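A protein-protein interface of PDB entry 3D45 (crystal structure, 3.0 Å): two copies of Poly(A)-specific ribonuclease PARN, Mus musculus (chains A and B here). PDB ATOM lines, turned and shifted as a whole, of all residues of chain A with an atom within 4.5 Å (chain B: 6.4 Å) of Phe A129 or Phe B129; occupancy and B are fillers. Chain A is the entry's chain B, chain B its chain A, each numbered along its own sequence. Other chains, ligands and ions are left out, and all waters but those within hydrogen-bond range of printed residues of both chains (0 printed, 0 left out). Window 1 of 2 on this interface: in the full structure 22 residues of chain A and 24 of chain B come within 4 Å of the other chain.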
ATOM      1  N   ARG A   7       2.084   5.711  25.167  1.00  0.00           N
ATOM      2  CA  ARG A   7       0.816   6.145  25.751  1.00  0.00           C
ATOM      3  C   ARG A   7       1.048   7.199  26.831  1.00  0.00           C
ATOM      4  O   ARG A   7       0.617   8.350  26.725  1.00  0.00           O
ATOM      5  CB  ARG A   7       0.123   4.930  26.361  1.00  0.00           C
ATOM      6  CG  ARG A   7      -1.368   5.063  26.601  1.00  0.00           C
ATOM      7  CD  ARG A   7      -1.919   3.771  27.192  1.00  0.00           C
ATOM      8  NE  ARG A   7      -1.557   2.608  26.375  1.00  0.00           N
ATOM      9  CZ  ARG A   7      -1.930   1.360  26.635  1.00  0.00           C
ATOM     10  NH1 ARG A   7      -2.666   1.119  27.708  1.00  0.00           N
ATOM     11  NH2 ARG A   7      -1.559   0.353  25.836  1.00  0.00           N
ATOM     12  N   PHE A  95      -1.526   1.344  19.402  1.00  0.00           N
ATOM     13  CA  PHE A  95      -2.285   0.130  19.743  1.00  0.00           C
ATOM     14  C   PHE A  95      -3.762   0.432  20.067  1.00  0.00           C
ATOM     15  O   PHE A  95      -4.043   1.241  20.955  1.00  0.00           O
ATOM     16  CB  PHE A  95      -1.614  -0.595  20.921  1.00  0.00           C
ATOM     17  CG  PHE A  95      -2.418  -1.728  21.455  1.00  0.00           C
ATOM     18  CD1 PHE A  95      -2.469  -2.936  20.776  1.00  0.00           C
ATOM     19  CD2 PHE A  95      -3.160  -1.580  22.623  1.00  0.00           C
ATOM     20  CE1 PHE A  95      -3.236  -3.980  21.250  1.00  0.00           C
ATOM     21  CE2 PHE A  95      -3.941  -2.633  23.106  1.00  0.00           C
ATOM     22  CZ  PHE A  95      -3.980  -3.832  22.417  1.00  0.00           C
ATOM     23  N   PHE A 108      -6.993  -7.529  15.154  1.00  0.00           N
ATOM     24  CA  PHE A 108      -5.979  -7.468  14.130  1.00  0.00           C
ATOM     25  C   PHE A 108      -5.287  -8.829  14.020  1.00  0.00           C
ATOM     26  O   PHE A 108      -5.523  -9.697  14.881  1.00  0.00           O
ATOM     27  CB  PHE A 108      -5.027  -6.331  14.450  1.00  0.00           C
ATOM     28  CG  PHE A 108      -4.362  -6.462  15.774  1.00  0.00           C
ATOM     29  CD1 PHE A 108      -3.213  -7.232  15.916  1.00  0.00           C
ATOM     30  CD2 PHE A 108      -4.865  -5.810  16.876  1.00  0.00           C
ATOM     31  CE1 PHE A 108      -2.570  -7.346  17.145  1.00  0.00           C
ATOM     32  CE2 PHE A 108      -4.238  -5.907  18.116  1.00  0.00           C
ATOM     33  CZ  PHE A 108      -3.084  -6.678  18.252  1.00  0.00           C
ATOM     34  N   ILE A 115       6.635 -11.275  12.859  1.00  0.00           N
ATOM     35  CA  ILE A 115       6.840 -11.074  14.275  1.00  0.00           C
ATOM     36  C   ILE A 115       8.242 -11.500  14.662  1.00  0.00           C
ATOM     37  O   ILE A 115       9.013 -10.696  15.230  1.00  0.00           O
ATOM     38  CB  ILE A 115       5.778 -11.784  15.100  1.00  0.00           C
ATOM     39  CG1 ILE A 115       4.393 -11.379  14.593  1.00  0.00           C
ATOM     40  CG2 ILE A 115       5.913 -11.416  16.580  1.00  0.00           C
ATOM     41  CD1 ILE A 115       3.995  -9.946  14.931  1.00  0.00           C
ATOM     42  N   ALA A 119      11.467  -9.509  16.081  1.00  0.00           N
ATOM     43  CA  ALA A 119      12.147  -9.957  17.281  1.00  0.00           C
ATOM     44  C   ALA A 119      13.645  -9.854  17.083  1.00  0.00           C
ATOM     45  O   ALA A 119      14.336  -9.281  17.912  1.00  0.00           O
ATOM     46  CB  ALA A 119      11.758 -11.369  17.639  1.00  0.00           C
ATOM     47  N   PHE A 125       7.905  -5.598  22.237  1.00  0.00           N
ATOM     48  CA  PHE A 125       6.475  -5.750  21.973  1.00  0.00           C
ATOM     49  C   PHE A 125       5.630  -5.202  23.101  1.00  0.00           C
ATOM     50  O   PHE A 125       4.470  -4.804  22.914  1.00  0.00           O
ATOM     51  CB  PHE A 125       6.140  -7.201  21.720  1.00  0.00           C
ATOM     52  CG  PHE A 125       6.728  -7.726  20.466  1.00  0.00           C
ATOM     53  CD1 PHE A 125       7.988  -8.317  20.465  1.00  0.00           C
ATOM     54  CD2 PHE A 125       6.034  -7.625  19.270  1.00  0.00           C
ATOM     55  CE1 PHE A 125       8.543  -8.829  19.268  1.00  0.00           C
ATOM     56  CE2 PHE A 125       6.569  -8.126  18.087  1.00  0.00           C
ATOM     57  CZ  PHE A 125       7.828  -8.729  18.080  1.00  0.00           C
ATOM     58  N   ASN A 126       6.234  -5.177  24.276  1.00  0.00           N
ATOM     59  CA  ASN A 126       5.586  -4.591  25.414  1.00  0.00           C
ATOM     60  C   ASN A 126       5.241  -3.116  25.201  1.00  0.00           C
ATOM     61  O   ASN A 126       4.200  -2.637  25.672  1.00  0.00           O
ATOM     62  CB  ASN A 126       6.450  -4.832  26.635  1.00  0.00           C
ATOM     63  CG  ASN A 126       6.195  -6.191  27.242  1.00  0.00           C
ATOM     64  OD1 ASN A 126       6.561  -7.241  26.706  1.00  0.00           O
ATOM     65  ND2 ASN A 126       5.530  -6.174  28.372  1.00  0.00           N
ATOM     66  N   LYS A 127       6.098  -2.416  24.448  1.00  0.00           N
ATOM     67  CA  LYS A 127       5.865  -1.029  24.046  1.00  0.00           C
ATOM     68  C   LYS A 127       4.572  -0.911  23.245  1.00  0.00           C
ATOM     69  O   LYS A 127       3.771   0.015  23.441  1.00  0.00           O
ATOM     70  CB  LYS A 127       7.034  -0.508  23.216  1.00  0.00           C
ATOM     71  CG  LYS A 127       8.312  -0.384  24.003  1.00  0.00           C
ATOM     72  CD  LYS A 127       9.211   0.729  23.466  1.00  0.00           C
ATOM     73  CE  LYS A 127      10.461   0.973  24.326  1.00  0.00           C
ATOM     74  NZ  LYS A 127      11.468  -0.133  24.214  1.00  0.00           N
ATOM     75  N   VAL A 128       4.354  -1.873  22.365  1.00  0.00           N
ATOM     76  CA  VAL A 128       3.164  -1.857  21.565  1.00  0.00           C
ATOM     77  C   VAL A 128       1.943  -2.227  22.377  1.00  0.00           C
ATOM     78  O   VAL A 128       0.962  -1.469  22.414  1.00  0.00           O
ATOM     79  CB  VAL A 128       3.291  -2.784  20.388  1.00  0.00           C
ATOM     80  CG1 VAL A 128       1.910  -3.061  19.778  1.00  0.00           C
ATOM     81  CG2 VAL A 128       4.274  -2.170  19.358  1.00  0.00           C
ATOM     82  N   PHE A 129       2.014  -3.370  23.052  1.00  0.00           N
ATOM     83  CA  PHE A 129       0.814  -3.985  23.594  1.00  0.00           C
ATOM     84  C   PHE A 129       0.442  -3.501  24.972  1.00  0.00           C
ATOM     85  O   PHE A 129      -0.729  -3.548  25.332  1.00  0.00           O
ATOM     86  CB  PHE A 129       0.915  -5.505  23.547  1.00  0.00           C
ATOM     87  CG  PHE A 129       0.945  -6.070  22.143  1.00  0.00           C
ATOM     88  CD1 PHE A 129       1.958  -6.936  21.745  1.00  0.00           C
ATOM     89  CD2 PHE A 129      -0.036  -5.735  21.216  1.00  0.00           C
ATOM     90  CE1 PHE A 129       1.985  -7.468  20.443  1.00  0.00           C
ATOM     91  CE2 PHE A 129      -0.003  -6.263  19.921  1.00  0.00           C
ATOM     92  CZ  PHE A 129       1.012  -7.127  19.541  1.00  0.00           C
ATOM     93  N   CYS A 130       1.422  -3.021  25.731  1.00  0.00           N
ATOM     94  CA  CYS A 130       1.143  -2.460  27.057  1.00  0.00           C
ATOM     95  C   CYS A 130       1.111  -0.961  27.008  1.00  0.00           C
ATOM     96  O   CYS A 130       0.342  -0.347  27.749  1.00  0.00           O
ATOM     97  CB  CYS A 130       2.178  -2.902  28.076  1.00  0.00           C
ATOM     98  SG  CYS A 130       2.521  -4.649  27.931  1.00  0.00           S
ATOM     99  N   SER A 131       1.929  -0.376  26.131  1.00  0.00           N
ATOM    100  CA  SER A 131       2.130   1.071  26.112  1.00  0.00           C
ATOM    101  C   SER A 131       1.766   1.751  24.805  1.00  0.00           C
ATOM    102  O   SER A 131       2.088   2.931  24.621  1.00  0.00           O
ATOM    103  CB  SER A 131       3.581   1.391  26.435  1.00  0.00           C
ATOM    104  OG  SER A 131       3.873   0.988  27.754  1.00  0.00           O
ATOM    105  N   ARG B   7      11.884 -20.505  25.496  1.00  0.00           N
ATOM    106  CA  ARG B   7      12.564 -21.262  24.446  1.00  0.00           C
ATOM    107  C   ARG B   7      13.964 -21.655  24.889  1.00  0.00           C
ATOM    108  O   ARG B   7      14.312 -22.831  24.892  1.00  0.00           O
ATOM    109  CB  ARG B   7      12.642 -20.419  23.180  1.00  0.00           C
ATOM    110  CG  ARG B   7      13.071 -21.146  21.941  1.00  0.00           C
ATOM    111  CD  ARG B   7      13.256 -20.126  20.811  1.00  0.00           C
ATOM    112  NE  ARG B   7      12.022 -19.375  20.606  1.00  0.00           N
ATOM    113  CZ  ARG B   7      11.870 -18.332  19.792  1.00  0.00           C
ATOM    114  NH1 ARG B   7      12.886 -17.882  19.071  1.00  0.00           N
ATOM    115  NH2 ARG B   7      10.688 -17.735  19.709  1.00  0.00           N
ATOM    116  N   SER B  34      -4.662 -15.234  22.985  1.00  0.00           N
ATOM    117  CA  SER B  34      -4.614 -14.036  22.156  1.00  0.00           C
ATOM    118  C   SER B  34      -5.908 -13.199  22.194  1.00  0.00           C
ATOM    119  O   SER B  34      -5.878 -11.971  21.954  1.00  0.00           O
ATOM    120  CB  SER B  34      -4.402 -14.507  20.735  1.00  0.00           C
ATOM    121  OG  SER B  34      -3.793 -13.505  19.988  1.00  0.00           O
ATOM    122  N   LEU B  67      -4.513 -17.365  19.560  1.00  0.00           N
ATOM    123  CA  LEU B  67      -3.355 -18.123  19.981  1.00  0.00           C
ATOM    124  C   LEU B  67      -3.289 -18.354  21.482  1.00  0.00           C
ATOM    125  O   LEU B  67      -3.332 -17.407  22.292  1.00  0.00           O
ATOM    126  CB  LEU B  67      -2.105 -17.387  19.559  1.00  0.00           C
ATOM    127  CG  LEU B  67      -0.925 -18.274  19.230  1.00  0.00           C
ATOM    128  CD1 LEU B  67      -1.321 -19.301  18.133  1.00  0.00           C
ATOM    129  CD2 LEU B  67       0.259 -17.357  18.811  1.00  0.00           C
ATOM    130  N   PHE B  69      -1.054 -18.702  24.074  1.00  0.00           N
ATOM    131  CA  PHE B  69       0.394 -18.352  24.117  1.00  0.00           C
ATOM    132  C   PHE B  69       1.062 -18.450  25.505  1.00  0.00           C
ATOM    133  O   PHE B  69       2.287 -18.239  25.666  1.00  0.00           O
ATOM    134  CB  PHE B  69       0.756 -17.035  23.349  1.00  0.00           C
ATOM    135  CG  PHE B  69      -0.062 -15.827  23.740  1.00  0.00           C
ATOM    136  CD1 PHE B  69      -0.561 -15.668  25.041  1.00  0.00           C
ATOM    137  CD2 PHE B  69      -0.298 -14.822  22.811  1.00  0.00           C
ATOM    138  CE1 PHE B  69      -1.319 -14.548  25.383  1.00  0.00           C
ATOM    139  CE2 PHE B  69      -1.061 -13.696  23.144  1.00  0.00           C
ATOM    140  CZ  PHE B  69      -1.567 -13.558  24.432  1.00  0.00           C
ATOM    141  N   PHE B  95       5.007 -20.110  21.228  1.00  0.00           N
ATOM    142  CA  PHE B  95       4.901 -19.281  20.004  1.00  0.00           C
ATOM    143  C   PHE B  95       5.324 -20.040  18.725  1.00  0.00           C
ATOM    144  O   PHE B  95       6.462 -20.553  18.637  1.00  0.00           O
ATOM    145  CB  PHE B  95       5.731 -17.992  20.131  1.00  0.00           C
ATOM    146  CG  PHE B  95       5.835 -17.199  18.859  1.00  0.00           C
ATOM    147  CD1 PHE B  95       4.775 -16.410  18.421  1.00  0.00           C
ATOM    148  CD2 PHE B  95       6.994 -17.216  18.111  1.00  0.00           C
ATOM    149  CE1 PHE B  95       4.850 -15.655  17.236  1.00  0.00           C
ATOM    150  CE2 PHE B  95       7.089 -16.463  16.909  1.00  0.00           C
ATOM    151  CZ  PHE B  95       6.003 -15.686  16.482  1.00  0.00           C
ATOM    152  N   PHE B 108      -2.161 -15.884  13.401  1.00  0.00           N
ATOM    153  CA  PHE B 108      -3.145 -15.883  14.489  1.00  0.00           C
ATOM    154  C   PHE B 108      -3.830 -14.550  14.634  1.00  0.00           C
ATOM    155  O   PHE B 108      -3.383 -13.526  14.107  1.00  0.00           O
ATOM    156  CB  PHE B 108      -2.522 -16.248  15.828  1.00  0.00           C
ATOM    157  CG  PHE B 108      -1.405 -15.370  16.237  1.00  0.00           C
ATOM    158  CD1 PHE B 108      -1.620 -14.322  17.114  1.00  0.00           C
ATOM    159  CD2 PHE B 108      -0.122 -15.605  15.783  1.00  0.00           C
ATOM    160  CE1 PHE B 108      -0.549 -13.492  17.509  1.00  0.00           C
ATOM    161  CE2 PHE B 108       0.941 -14.793  16.169  1.00  0.00           C
ATOM    162  CZ  PHE B 108       0.732 -13.735  17.028  1.00  0.00           C
ATOM    163  N   CYS B 110      -5.428 -11.468  17.151  1.00  0.00           N
ATOM    164  CA  CYS B 110      -5.485 -10.822  18.465  1.00  0.00           C
ATOM    165  C   CYS B 110      -6.727  -9.967  18.704  1.00  0.00           C
ATOM    166  O   CYS B 110      -7.089  -9.144  17.877  1.00  0.00           O
ATOM    167  CB  CYS B 110      -4.335  -9.860  18.664  1.00  0.00           C
ATOM    168  SG  CYS B 110      -2.764 -10.548  18.606  1.00  0.00           S
ATOM    169  N   ILE B 115      -5.812  -8.479  24.798  1.00  0.00           N
ATOM    170  CA  ILE B 115      -4.444  -7.972  24.882  1.00  0.00           C
ATOM    171  C   ILE B 115      -4.353  -6.918  25.972  1.00  0.00           C
ATOM    172  O   ILE B 115      -3.588  -7.084  26.915  1.00  0.00           O
ATOM    173  CB  ILE B 115      -3.895  -7.432  23.539  1.00  0.00           C
ATOM    174  CG1 ILE B 115      -3.502  -8.595  22.624  1.00  0.00           C
ATOM    175  CG2 ILE B 115      -2.687  -6.510  23.773  1.00  0.00           C
ATOM    176  CD1 ILE B 115      -2.518  -9.548  23.250  1.00  0.00           C
ATOM    177  N   ASP B 116      -5.165  -5.867  25.867  1.00  0.00           N
ATOM    178  CA  ASP B 116      -5.108  -4.780  26.833  1.00  0.00           C
ATOM    179  C   ASP B 116      -5.337  -5.289  28.224  1.00  0.00           C
ATOM    180  O   ASP B 116      -4.709  -4.777  29.151  1.00  0.00           O
ATOM    181  CB  ASP B 116      -6.106  -3.672  26.545  1.00  0.00           C
ATOM    182  CG  ASP B 116      -6.297  -2.743  27.739  1.00  0.00           C
ATOM    183  OD1 ASP B 116      -5.338  -2.003  28.082  1.00  0.00           O
ATOM    184  OD2 ASP B 116      -7.409  -2.782  28.331  1.00  0.00           O
ATOM    185  N   ALA B 119      -2.211  -6.841  29.410  1.00  0.00           N
ATOM    186  CA  ALA B 119      -1.318  -5.752  29.667  1.00  0.00           C
ATOM    187  C   ALA B 119      -1.484  -5.312  31.133  1.00  0.00           C
ATOM    188  O   ALA B 119      -0.506  -5.287  31.905  1.00  0.00           O
ATOM    189  CB  ALA B 119      -1.625  -4.614  28.709  1.00  0.00           C
ATOM    190  N   ASP B 124       4.120 -10.225  29.960  1.00  0.00           N
ATOM    191  CA  ASP B 124       5.333  -9.813  29.272  1.00  0.00           C
ATOM    192  C   ASP B 124       5.315 -10.387  27.889  1.00  0.00           C
ATOM    193  O   ASP B 124       5.727 -11.526  27.706  1.00  0.00           O
ATOM    194  CB  ASP B 124       6.542 -10.391  29.986  1.00  0.00           C
ATOM    195  CG  ASP B 124       7.827  -9.646  29.661  1.00  0.00           C
ATOM    196  OD1 ASP B 124       8.341  -9.750  28.526  1.00  0.00           O
ATOM    197  OD2 ASP B 124       8.338  -8.951  30.567  1.00  0.00           O
ATOM    198  N   PHE B 125       4.866  -9.612  26.903  1.00  0.00           N
ATOM    199  CA  PHE B 125       4.637 -10.174  25.570  1.00  0.00           C
ATOM    200  C   PHE B 125       5.921 -10.577  24.867  1.00  0.00           C
ATOM    201  O   PHE B 125       5.916 -11.479  24.029  1.00  0.00           O
ATOM    202  CB  PHE B 125       3.819  -9.232  24.713  1.00  0.00           C
ATOM    203  CG  PHE B 125       2.479  -8.947  25.268  1.00  0.00           C
ATOM    204  CD1 PHE B 125       2.264  -7.803  26.043  1.00  0.00           C
ATOM    205  CD2 PHE B 125       1.425  -9.822  25.040  1.00  0.00           C
ATOM    206  CE1 PHE B 125       1.009  -7.519  26.566  1.00  0.00           C
ATOM    207  CE2 PHE B 125       0.162  -9.560  25.555  1.00  0.00           C
ATOM    208  CZ  PHE B 125      -0.047  -8.399  26.326  1.00  0.00           C
ATOM    209  N   ASN B 126       7.012  -9.903  25.207  1.00  0.00           N
ATOM    210  CA  ASN B 126       8.310 -10.277  24.704  1.00  0.00           C
ATOM    211  C   ASN B 126       8.614 -11.737  24.942  1.00  0.00           C
ATOM    212  O   ASN B 126       9.181 -12.413  24.074  1.00  0.00           O
ATOM    213  CB  ASN B 126       9.370  -9.432  25.348  1.00  0.00           C
ATOM    214  CG  ASN B 126       9.644  -8.250  24.561  1.00  0.00           C
ATOM    215  OD1 ASN B 126       9.069  -7.192  24.801  1.00  0.00           O
ATOM    216  ND2 ASN B 126      10.460  -8.410  23.531  1.00  0.00           N
ATOM    217  N   LYS B 127       8.229 -12.236  26.116  1.00  0.00           N
ATOM    218  CA  LYS B 127       8.466 -13.628  26.439  1.00  0.00           C
ATOM    219  C   LYS B 127       7.695 -14.509  25.472  1.00  0.00           C
ATOM    220  O   LYS B 127       8.148 -15.600  25.156  1.00  0.00           O
ATOM    221  CB  LYS B 127       8.078 -13.960  27.877  1.00  0.00           C
ATOM    222  CG  LYS B 127       9.074 -13.553  28.925  1.00  0.00           C
ATOM    223  CD  LYS B 127       8.419 -13.706  30.291  1.00  0.00           C
ATOM    224  CE  LYS B 127       9.356 -13.398  31.472  1.00  0.00           C
ATOM    225  NZ  LYS B 127       9.653 -11.932  31.578  1.00  0.00           N
ATOM    226  N   VAL B 128       6.541 -14.045  24.990  1.00  0.00           N
ATOM    227  CA  VAL B 128       5.774 -14.851  24.048  1.00  0.00           C
ATOM    228  C   VAL B 128       6.319 -14.725  22.661  1.00  0.00           C
ATOM    229  O   VAL B 128       6.565 -15.748  22.038  1.00  0.00           O
ATOM    230  CB  VAL B 128       4.280 -14.563  24.009  1.00  0.00           C
ATOM    231  CG1 VAL B 128       3.661 -15.369  22.918  1.00  0.00           C
ATOM    232  CG2 VAL B 128       3.626 -14.924  25.315  1.00  0.00           C
ATOM    233  N   PHE B 129       6.519 -13.496  22.166  1.00  0.00           N
ATOM    234  CA  PHE B 129       6.977 -13.295  20.751  1.00  0.00           C
ATOM    235  C   PHE B 129       8.487 -13.390  20.473  1.00  0.00           C
ATOM    236  O   PHE B 129       8.889 -13.692  19.360  1.00  0.00           O
ATOM    237  CB  PHE B 129       6.414 -12.016  20.166  1.00  0.00           C
ATOM    238  CG  PHE B 129       4.943 -11.875  20.360  1.00  0.00           C
ATOM    239  CD1 PHE B 129       4.417 -10.744  20.979  1.00  0.00           C
ATOM    240  CD2 PHE B 129       4.071 -12.877  19.932  1.00  0.00           C
ATOM    241  CE1 PHE B 129       3.042 -10.609  21.156  1.00  0.00           C
ATOM    242  CE2 PHE B 129       2.698 -12.747  20.103  1.00  0.00           C
ATOM    243  CZ  PHE B 129       2.182 -11.625  20.717  1.00  0.00           C
ATOM    244  N   CYS B 130       9.311 -13.145  21.482  1.00  0.00           N
ATOM    245  CA  CYS B 130      10.735 -13.252  21.289  1.00  0.00           C
ATOM    246  C   CYS B 130      11.258 -14.588  21.766  1.00  0.00           C
ATOM    247  O   CYS B 130      12.235 -15.113  21.225  1.00  0.00           O
ATOM    248  CB  CYS B 130      11.457 -12.154  22.047  1.00  0.00           C
ATOM    249  SG  CYS B 130      10.945 -10.548  21.530  1.00  0.00           S
ATOM    250  N   SER B 131      10.606 -15.134  22.780  1.00  0.00           N
ATOM    251  CA  SER B 131      11.178 -16.242  23.512  1.00  0.00           C
ATOM    252  C   SER B 131      10.222 -17.390  23.640  1.00  0.00           C
ATOM    253  O   SER B 131      10.453 -18.292  24.425  1.00  0.00           O
ATOM    254  CB  SER B 131      11.605 -15.771  24.904  1.00  0.00           C
ATOM    255  OG  SER B 131      12.710 -14.906  24.816  1.00  0.00           O
ATOM    256  N   GLY B 132       9.138 -17.361  22.883  1.00  0.00           N
ATOM    257  CA  GLY B 132       8.115 -18.407  22.995  1.00  0.00           C
ATOM    258  C   GLY B 132       8.646 -19.718  22.466  1.00  0.00           C
ATOM    259  O   GLY B 132       9.460 -19.723  21.559  1.00  0.00           O
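The side-chain amide oxygen of Asn A126 sits at hydrogen-bond distance from the backbone NH of Phe B125, 2.9 Å away. The backbone NH (N) of Asn B126 sits at hydrogen-bond distance from the side-chain amide oxygen (OD1) of Asn A126 (3.1 Å). The side-chain amide oxygen (OD1) of Asn B126 sits at hydrogen-bond distance from the backbone NH (N) of Phe A125 (3.2 Å). The backbone carbonyl oxygen (O) of Phe A108 is in hydrogen-bond range of the backbone NH (N) of Cys B110 (2.9 Å).
Phe A129 touches just these residues of chain B: Ile B115, Ala B119, Phe B125 and Phe B129. Of chain A, only Ile A115 (3.7 Å), Phe A125 (3.8 Å) and Phe A129 (3.4 Å) come within 4 Å of Phe B129. Of the printed residues of chain A, Asn B126 touches Phe A125 and Asn A126. Of the printed residues of chain B, Phe A125 touches Asn B126 (3.2 Å), Phe B129 (3.8 Å) and Cys B130 (3.7 Å). Printed residues of chain B within 4 Å of Phe A95: Ile B115. The nearest residue of chain A that does not touch Phe B129 is Ala A119 (4.1 Å).
Phe A95 touches Ile B115, but with the chains exchanged Ile A115 does not touch Phe B95 (4.1 Å). Ile A115 touches Phe B129, and with the chains exchanged Phe A129 touches Ile B115. Asn B126 touches its own counterpart, Asn A126. Cys A130 touches Ala B119, but with the chains exchanged Ala A119 does not touch Cys B130 (4.1 Å). Of the 15 pairs that touch across the chains among the printed residues, 10 have their exchanged pair printed and touching as well.
Phe A95 touches Ile B115. Ile A115 touches Phe B129 (CG2 to CB, 3.7 Å). CD1 of Phe B129 touches CG of Phe A125 (3.8 Å). Phe A125 touches Cys B130 (CE1 to SG, 3.7 Å). Asp B124 touches Asn A126 (OD1 to OD1, 3.6 Å). CB of Phe A129 touches CG2 of Ile B115 (3.7 Å). CB of Ala B119 touches O of Phe A129, at 3.7 Å. Phe A129 touches Phe B129 (CE1 to CE1, 3.4 Å). Ala B119 touches Cys A130. Cys A130 touches Phe B125 (SG to CE1, 3.5 Å).
Of the 19 printed residues of chain B, 8 touch a printed residue of chain A. Hydrophobic or aromatic side chains of chain B that line the printed part of chain A: Ile B115, Ala B119, Phe B125 and Phe B129. Hydrophobic or aromatic side chains of chain A within 4 Å of the printed part of chain B: Phe A95, Phe A108, Ile A115, Phe A125 and Phe A129.
The backbone carbonyl oxygen (O) of Asn B126 lies within hydrogen-bond range of the backbone NH (N) of Ser B131 (3.3 Å). The backbone carbonyl oxygen (O) of Cys A130 sits at hydrogen-bond distance from the guanidinium group (NH2) of Arg A7 (2.8 Å). The side-chain amide nitrogen of Asn B126 sits at hydrogen-bond distance from the side-chain sulfur of Cys B130 (3.0 Å). NZ of Lys B127 is in salt-bridge range of OD2 of Asp B124, 3.4 Å away. N of Ser A131 is in hydrogen-bond range of O of Asn A126. The side-chain hydroxyl (OG) of Ser B34 is in hydrogen-bond range of the side-chain sulfur (SG) of Cys B110 (3.4 Å).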
